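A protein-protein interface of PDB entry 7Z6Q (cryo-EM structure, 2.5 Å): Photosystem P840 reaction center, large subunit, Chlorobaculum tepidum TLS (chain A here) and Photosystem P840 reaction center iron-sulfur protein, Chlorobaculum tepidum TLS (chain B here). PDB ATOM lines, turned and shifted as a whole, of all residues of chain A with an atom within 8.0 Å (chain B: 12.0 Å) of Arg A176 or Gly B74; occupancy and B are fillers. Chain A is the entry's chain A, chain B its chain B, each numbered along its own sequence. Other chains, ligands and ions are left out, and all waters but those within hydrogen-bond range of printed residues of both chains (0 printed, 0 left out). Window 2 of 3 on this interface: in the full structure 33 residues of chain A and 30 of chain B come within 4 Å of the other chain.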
ATOM      1  N   LEU A 169       9.739  30.854  -3.422  1.00  0.00           N
ATOM      2  CA  LEU A 169       9.788  29.392  -3.467  1.00  0.00           C
ATOM      3  C   LEU A 169       8.500  28.786  -2.900  1.00  0.00           C
ATOM      4  O   LEU A 169       8.470  28.092  -1.885  1.00  0.00           O
ATOM      5  CB  LEU A 169      11.046  28.901  -2.754  1.00  0.00           C
ATOM      6  CG  LEU A 169      11.247  28.908  -1.233  1.00  0.00           C
ATOM      7  CD1 LEU A 169      12.499  28.127  -0.880  1.00  0.00           C
ATOM      8  CD2 LEU A 169      11.314  30.320  -0.668  1.00  0.00           C
ATOM      9  N   THR A 170       7.409  29.045  -3.618  1.00  0.00           N
ATOM     10  CA  THR A 170       6.076  28.618  -3.218  1.00  0.00           C
ATOM     11  C   THR A 170       5.642  27.399  -4.026  1.00  0.00           C
ATOM     12  O   THR A 170       5.761  27.382  -5.254  1.00  0.00           O
ATOM     13  CB  THR A 170       5.068  29.762  -3.385  1.00  0.00           C
ATOM     14  OG1 THR A 170       3.763  29.322  -2.989  1.00  0.00           O
ATOM     15  CG2 THR A 170       5.026  30.268  -4.827  1.00  0.00           C
ATOM     16  N   ASN A 171       5.152  26.382  -3.336  1.00  0.00           N
ATOM     17  CA  ASN A 171       4.628  25.211  -4.026  1.00  0.00           C
ATOM     18  C   ASN A 171       3.334  25.592  -4.734  1.00  0.00           C
ATOM     19  O   ASN A 171       2.388  26.038  -4.072  1.00  0.00           O
ATOM     20  CB  ASN A 171       4.394  24.077  -3.030  1.00  0.00           C
ATOM     21  CG  ASN A 171       4.031  22.768  -3.703  1.00  0.00           C
ATOM     22  OD1 ASN A 171       2.987  22.655  -4.345  1.00  0.00           O
ATOM     23  ND2 ASN A 171       4.890  21.767  -3.552  1.00  0.00           N
ATOM     24  N   PRO A 172       3.246  25.457  -6.060  1.00  0.00           N
ATOM     25  CA  PRO A 172       2.008  25.852  -6.750  1.00  0.00           C
ATOM     26  C   PRO A 172       0.839  24.922  -6.484  1.00  0.00           C
ATOM     27  O   PRO A 172      -0.313  25.339  -6.654  1.00  0.00           O
ATOM     28  CB  PRO A 172       2.404  25.839  -8.235  1.00  0.00           C
ATOM     29  CG  PRO A 172       3.903  25.714  -8.259  1.00  0.00           C
ATOM     30  CD  PRO A 172       4.285  25.012  -7.000  1.00  0.00           C
ATOM     31  N   PHE A 173       1.095  23.679  -6.077  1.00  0.00           N
ATOM     32  CA  PHE A 173       0.011  22.745  -5.790  1.00  0.00           C
ATOM     33  C   PHE A 173      -0.531  22.958  -4.382  1.00  0.00           C
ATOM     34  O   PHE A 173      -1.713  23.268  -4.198  1.00  0.00           O
ATOM     35  CB  PHE A 173       0.500  21.308  -5.978  1.00  0.00           C
ATOM     36  CG  PHE A 173       1.279  21.094  -7.247  1.00  0.00           C
ATOM     37  CD1 PHE A 173       0.850  21.649  -8.443  1.00  0.00           C
ATOM     38  CD2 PHE A 173       2.445  20.346  -7.243  1.00  0.00           C
ATOM     39  CE1 PHE A 173       1.566  21.458  -9.609  1.00  0.00           C
ATOM     40  CE2 PHE A 173       3.166  20.153  -8.407  1.00  0.00           C
ATOM     41  CZ  PHE A 173       2.725  20.710  -9.592  1.00  0.00           C
ATOM     42  N   THR A 174       0.324  22.799  -3.375  1.00  0.00           N
ATOM     43  CA  THR A 174      -0.030  23.111  -1.995  1.00  0.00           C
ATOM     44  C   THR A 174       0.390  24.550  -1.718  1.00  0.00           C
ATOM     45  O   THR A 174       1.582  24.868  -1.747  1.00  0.00           O
ATOM     46  CB  THR A 174       0.643  22.141  -1.026  1.00  0.00           C
ATOM     47  OG1 THR A 174       2.037  22.455  -0.920  1.00  0.00           O
ATOM     48  CG2 THR A 174       0.490  20.710  -1.515  1.00  0.00           C
ATOM     49  N   GLY A 175      -0.585  25.410  -1.424  1.00  0.00           N
ATOM     50  CA  GLY A 175      -0.367  26.844  -1.323  1.00  0.00           C
ATOM     51  C   GLY A 175       0.775  27.298  -0.433  1.00  0.00           C
ATOM     52  O   GLY A 175       1.184  28.461  -0.494  1.00  0.00           O
ATOM     53  N   ARG A 176       1.203  26.393   0.452  1.00  0.00           N
ATOM     54  CA  ARG A 176       2.245  26.679   1.472  1.00  0.00           C
ATOM     55  C   ARG A 176       3.636  26.784   0.841  1.00  0.00           C
ATOM     56  O   ARG A 176       3.989  25.921   0.012  1.00  0.00           O
ATOM     57  CB  ARG A 176       2.227  25.604   2.564  1.00  0.00           C
ATOM     58  CG  ARG A 176       2.283  24.179   2.033  1.00  0.00           C
ATOM     59  CD  ARG A 176       3.222  23.298   2.836  1.00  0.00           C
ATOM     60  NE  ARG A 176       3.524  22.045   2.156  1.00  0.00           N
ATOM     61  CZ  ARG A 176       4.618  21.827   1.434  1.00  0.00           C
ATOM     62  NH1 ARG A 176       4.720  20.731   0.703  1.00  0.00           N
ATOM     63  NH2 ARG A 176       5.603  22.708   1.443  1.00  0.00           N
ATOM     64  N   CYS A 177       4.380  27.819   1.240  1.00  0.00           N
ATOM     65  CA  CYS A 177       5.780  28.047   0.792  1.00  0.00           C
ATOM     66  C   CYS A 177       6.744  27.311   1.725  1.00  0.00           C
ATOM     67  O   CYS A 177       6.288  26.761   2.725  1.00  0.00           O
ATOM     68  CB  CYS A 177       6.124  29.528   0.832  1.00  0.00           C
ATOM     69  SG  CYS A 177       5.150  30.497  -0.345  1.00  0.00           S
ATOM     70  N   GLY A 178       8.035  27.333   1.404  1.00  0.00           N
ATOM     71  CA  GLY A 178       9.041  26.632   2.220  1.00  0.00           C
ATOM     72  C   GLY A 178      10.049  27.598   2.808  1.00  0.00           C
ATOM     73  O   GLY A 178      10.089  28.752   2.363  1.00  0.00           O
ATOM     74  N   ASN A 179      10.826  27.124   3.782  1.00  0.00           N
ATOM     75  CA  ASN A 179      11.848  27.908   4.464  1.00  0.00           C
ATOM     76  C   ASN A 179      13.224  27.423   4.029  1.00  0.00           C
ATOM     77  O   ASN A 179      13.499  26.220   4.059  1.00  0.00           O
ATOM     78  CB  ASN A 179      11.695  27.794   5.984  1.00  0.00           C
ATOM     79  CG  ASN A 179      12.739  28.598   6.744  1.00  0.00           C
ATOM     80  OD1 ASN A 179      13.858  28.135   6.961  1.00  0.00           O
ATOM     81  ND2 ASN A 179      12.369  29.802   7.168  1.00  0.00           N
ATOM     82  N   ARG A 184      12.369  20.114   5.456  1.00  0.00           N
ATOM     83  CA  ARG A 184      12.353  18.640   5.675  1.00  0.00           C
ATOM     84  C   ARG A 184      13.298  17.893   4.726  1.00  0.00           C
ATOM     85  O   ARG A 184      13.705  16.772   5.101  1.00  0.00           O
ATOM     86  CB  ARG A 184      10.924  18.101   5.547  1.00  0.00           C
ATOM     87  CG  ARG A 184      10.737  16.695   6.097  1.00  0.00           C
ATOM     88  CD  ARG A 184       9.329  16.456   6.607  1.00  0.00           C
ATOM     89  NE  ARG A 184       8.314  16.927   5.676  1.00  0.00           N
ATOM     90  CZ  ARG A 184       7.404  16.153   5.098  1.00  0.00           C
ATOM     91  NH1 ARG A 184       7.378  14.856   5.357  1.00  0.00           N
ATOM     92  NH2 ARG A 184       6.523  16.676   4.265  1.00  0.00           N
ATOM     93  N   GLY B  67       1.849  35.811  16.291  1.00  0.00           N
ATOM     94  CA  GLY B  67       2.088  35.232  14.986  1.00  0.00           C
ATOM     95  C   GLY B  67       3.566  35.229  14.669  1.00  0.00           C
ATOM     96  O   GLY B  67       4.124  36.225  14.200  1.00  0.00           O
ATOM     97  N   VAL B  68       4.205  34.091  14.925  1.00  0.00           N
ATOM     98  CA  VAL B  68       5.650  33.939  14.810  1.00  0.00           C
ATOM     99  C   VAL B  68       5.889  32.663  14.015  1.00  0.00           C
ATOM    100  O   VAL B  68       5.797  31.557  14.560  1.00  0.00           O
ATOM    101  CB  VAL B  68       6.343  33.881  16.176  1.00  0.00           C
ATOM    102  CG1 VAL B  68       7.833  33.647  16.007  1.00  0.00           C
ATOM    103  CG2 VAL B  68       6.090  35.162  16.954  1.00  0.00           C
ATOM    104  N   THR B  69       6.191  32.810  12.730  1.00  0.00           N
ATOM    105  CA  THR B  69       6.474  31.688  11.841  1.00  0.00           C
ATOM    106  C   THR B  69       7.938  31.807  11.430  1.00  0.00           C
ATOM    107  O   THR B  69       8.261  32.414  10.407  1.00  0.00           O
ATOM    108  CB  THR B  69       5.542  31.690  10.632  1.00  0.00           C
ATOM    109  OG1 THR B  69       5.683  32.928   9.921  1.00  0.00           O
ATOM    110  CG2 THR B  69       4.098  31.534  11.079  1.00  0.00           C
ATOM    111  N   LEU B  70       8.826  31.231  12.248  1.00  0.00           N
ATOM    112  CA  LEU B  70      10.291  31.342  12.006  1.00  0.00           C
ATOM    113  C   LEU B  70      10.897  30.015  11.532  1.00  0.00           C
ATOM    114  O   LEU B  70      11.769  30.063  10.642  1.00  0.00           O
ATOM    115  CB  LEU B  70      10.969  31.824  13.292  1.00  0.00           C
ATOM    116  CG  LEU B  70      10.787  33.306  13.616  1.00  0.00           C
ATOM    117  CD1 LEU B  70      11.660  33.715  14.793  1.00  0.00           C
ATOM    118  CD2 LEU B  70      11.093  34.168  12.401  1.00  0.00           C
ATOM    119  N   GLY B  71      10.464  28.879  12.092  1.00  0.00           N
ATOM    120  CA  GLY B  71      11.042  27.610  11.703  1.00  0.00           C
ATOM    121  C   GLY B  71      10.338  26.965  10.532  1.00  0.00           C
ATOM    122  O   GLY B  71       9.969  27.645   9.568  1.00  0.00           O
ATOM    123  N   ARG B  72      10.255  25.630  10.596  1.00  0.00           N
ATOM    124  CA  ARG B  72       9.579  24.796   9.568  1.00  0.00           C
ATOM    125  C   ARG B  72       8.092  25.144   9.626  1.00  0.00           C
ATOM    126  O   ARG B  72       7.395  24.635  10.525  1.00  0.00           O
ATOM    127  CB  ARG B  72       9.813  23.308   9.846  1.00  0.00           C
ATOM    128  CG  ARG B  72       9.001  22.373   8.963  1.00  0.00           C
ATOM    129  CD  ARG B  72       9.637  21.002   8.839  1.00  0.00           C
ATOM    130  NE  ARG B  72      11.089  21.075   8.743  1.00  0.00           N
ATOM    131  CZ  ARG B  72      11.928  20.632   9.673  1.00  0.00           C
ATOM    132  NH1 ARG B  72      11.460  20.081  10.778  1.00  0.00           N
ATOM    133  NH2 ARG B  72      13.231  20.744   9.493  1.00  0.00           N
ATOM    134  N   SER B  73       7.641  25.984   8.695  1.00  0.00           N
ATOM    135  CA  SER B  73       6.239  26.472   8.705  1.00  0.00           C
ATOM    136  C   SER B  73       5.845  26.692   7.240  1.00  0.00           C
ATOM    137  O   SER B  73       6.739  26.961   6.410  1.00  0.00           O
ATOM    138  CB  SER B  73       5.952  27.691   9.541  1.00  0.00           C
ATOM    139  OG  SER B  73       6.881  28.724   9.260  1.00  0.00           O
ATOM    140  N   GLY B  74       4.575  26.442   6.917  1.00  0.00           N
ATOM    141  CA  GLY B  74       4.093  26.596   5.532  1.00  0.00           C
ATOM    142  C   GLY B  74       3.882  28.055   5.194  1.00  0.00           C
ATOM    143  O   GLY B  74       3.473  28.348   4.061  1.00  0.00           O
ATOM    144  N   VAL B  75       4.225  28.940   6.133  1.00  0.00           N
ATOM    145  CA  VAL B  75       4.058  30.409   5.925  1.00  0.00           C
ATOM    146  C   VAL B  75       5.283  30.964   5.194  1.00  0.00           C
ATOM    147  O   VAL B  75       6.401  30.469   5.435  1.00  0.00           O
ATOM    148  CB  VAL B  75       3.819  31.145   7.254  1.00  0.00           C
ATOM    149  CG1 VAL B  75       3.381  32.583   7.021  1.00  0.00           C
ATOM    150  CG2 VAL B  75       2.811  30.410   8.121  1.00  0.00           C
ATOM    151  N   ARG B  76       5.092  31.981   4.345  1.00  0.00           N
ATOM    152  CA  ARG B  76       6.189  32.632   3.576  1.00  0.00           C
ATOM    153  C   ARG B  76       7.015  33.555   4.489  1.00  0.00           C
ATOM    154  O   ARG B  76       6.403  34.331   5.247  1.00  0.00           O
ATOM    155  CB  ARG B  76       5.570  33.412   2.412  1.00  0.00           C
ATOM    156  CG  ARG B  76       6.537  34.307   1.652  1.00  0.00           C
ATOM    157  CD  ARG B  76       6.023  34.579   0.251  1.00  0.00           C
ATOM    158  NE  ARG B  76       6.882  35.467  -0.518  1.00  0.00           N
ATOM    159  CZ  ARG B  76       8.123  35.179  -0.889  1.00  0.00           C
ATOM    160  NH1 ARG B  76       8.823  36.054  -1.590  1.00  0.00           N
ATOM    161  NH2 ARG B  76       8.661  34.020  -0.555  1.00  0.00           N
ATOM    162  N   GLN B  77       8.350  33.460   4.415  1.00  0.00           N
ATOM    163  CA  GLN B  77       9.306  34.291   5.208  1.00  0.00           C
ATOM    164  C   GLN B  77       9.520  35.650   4.521  1.00  0.00           C
ATOM    165  O   GLN B  77       9.014  35.825   3.395  1.00  0.00           O
ATOM    166  CB  GLN B  77      10.627  33.557   5.451  1.00  0.00           C
ATOM    167  CG  GLN B  77      10.498  32.326   6.337  1.00  0.00           C
ATOM    168  CD  GLN B  77       9.966  32.626   7.717  1.00  0.00           C
ATOM    169  OE1 GLN B  77      10.317  33.625   8.338  1.00  0.00           O
ATOM    170  NE2 GLN B  77       9.100  31.757   8.210  1.00  0.00           N
ATOM    171  N   GLU B  78      10.266  36.557   5.144  1.00  0.00           N
ATOM    172  CA  GLU B  78      10.506  37.876   4.562  1.00  0.00           C
ATOM    173  C   GLU B  78      11.867  38.018   3.872  1.00  0.00           C
ATOM    174  O   GLU B  78      12.909  38.037   4.526  1.00  0.00           O
ATOM    175  CB  GLU B  78      10.336  38.967   5.623  1.00  0.00           C
ATOM    176  CG  GLU B  78      11.509  39.097   6.582  1.00  0.00           C
ATOM    177  CD  GLU B  78      11.808  37.804   7.314  1.00  0.00           C
ATOM    178  OE1 GLU B  78      10.868  37.015   7.541  1.00  0.00           O
ATOM    179  OE2 GLU B  78      12.986  37.577   7.665  1.00  0.00           O
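The backbone carbonyl oxygen (O) of Gly B74 sits at hydrogen-bond distance from the backbone NH (N) of Cys A177, at 3.0 Å.
SG of Cys A177 lies close to OG1 of Thr A170, at 3.2 Å.
NE of Arg A176 sits close to OG1 of Thr A174 (3.4 Å).
O of Thr B69 lies within hydrogen-bond range of NE2 of Gln B77 (2.4 Å).
The backbone carbonyl oxygen of Gly B71 sits at hydrogen-bond distance from the side-chain hydroxyl of Ser B73 (3.3 Å).
Arg A176 touches Gly B74 (CA to O, 3.3 Å).
Cys A177 touches Ser B73.
Asn A179 touches Leu B70.
Gly B71 touches Asn A179.
Asn A179 touches Gln B77 (ND2 to CG, 3.2 Å).
Arg B72 touches Arg A184 (NE to N, 3.7 Å).
Thr A170 touches none of the printed residues of chain B.
Pro A172 touches none of the printed residues of chain B.
No residue of chain B comes within 4 Å of Thr A174.
No residue of chain B comes within 4 Å of Gly A175.
Of chain B, only Gly B74 (3.3 Å) comes within 4 Å of Arg A176.
Cys A177 touches just these residues of chain B: Ser B73 (3.7 Å) and Gly B74 (3.0 Å).
No residue of chain B comes within 4 Å of Gly A178.
Of the printed residues of chain B, Arg A184 touches Arg B72 (3.7 Å).
Gly B67 touches none of the printed residues of chain A.
Printed residues of chain A within 4 Å of Leu B70: Asn A179.
Printed residues of chain A within 4 Å of Gly B71: Asn A179.
Printed residues of chain A within 4 Å of Ser B73: Cys A177 (3.7 Å).
Of chain A, only Arg A176 and Cys A177 come within 4 Å of Gly B74.
Of the printed residues of chain A, Gln B77 touches Asn A179 (3.2 Å).
The nearest residue of chain B that does not touch Arg A176 is Val B75 (5.3 Å).
The nearest residue of chain A that does not touch Gly B74 is Gly A175 (5.1 Å).
Printed residues of chain B that touch a printed residue of chain A: Leu B70, Gly B71, Arg B72, Ser B73, Gly B74 and Gln B77.
Among the printed residues, 7 pairs touch across the chains.
Among the printed residues, no Asp or Glu carboxylate lies within 4 Å of a Lys or Arg side-chain nitrogen of the other chain.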
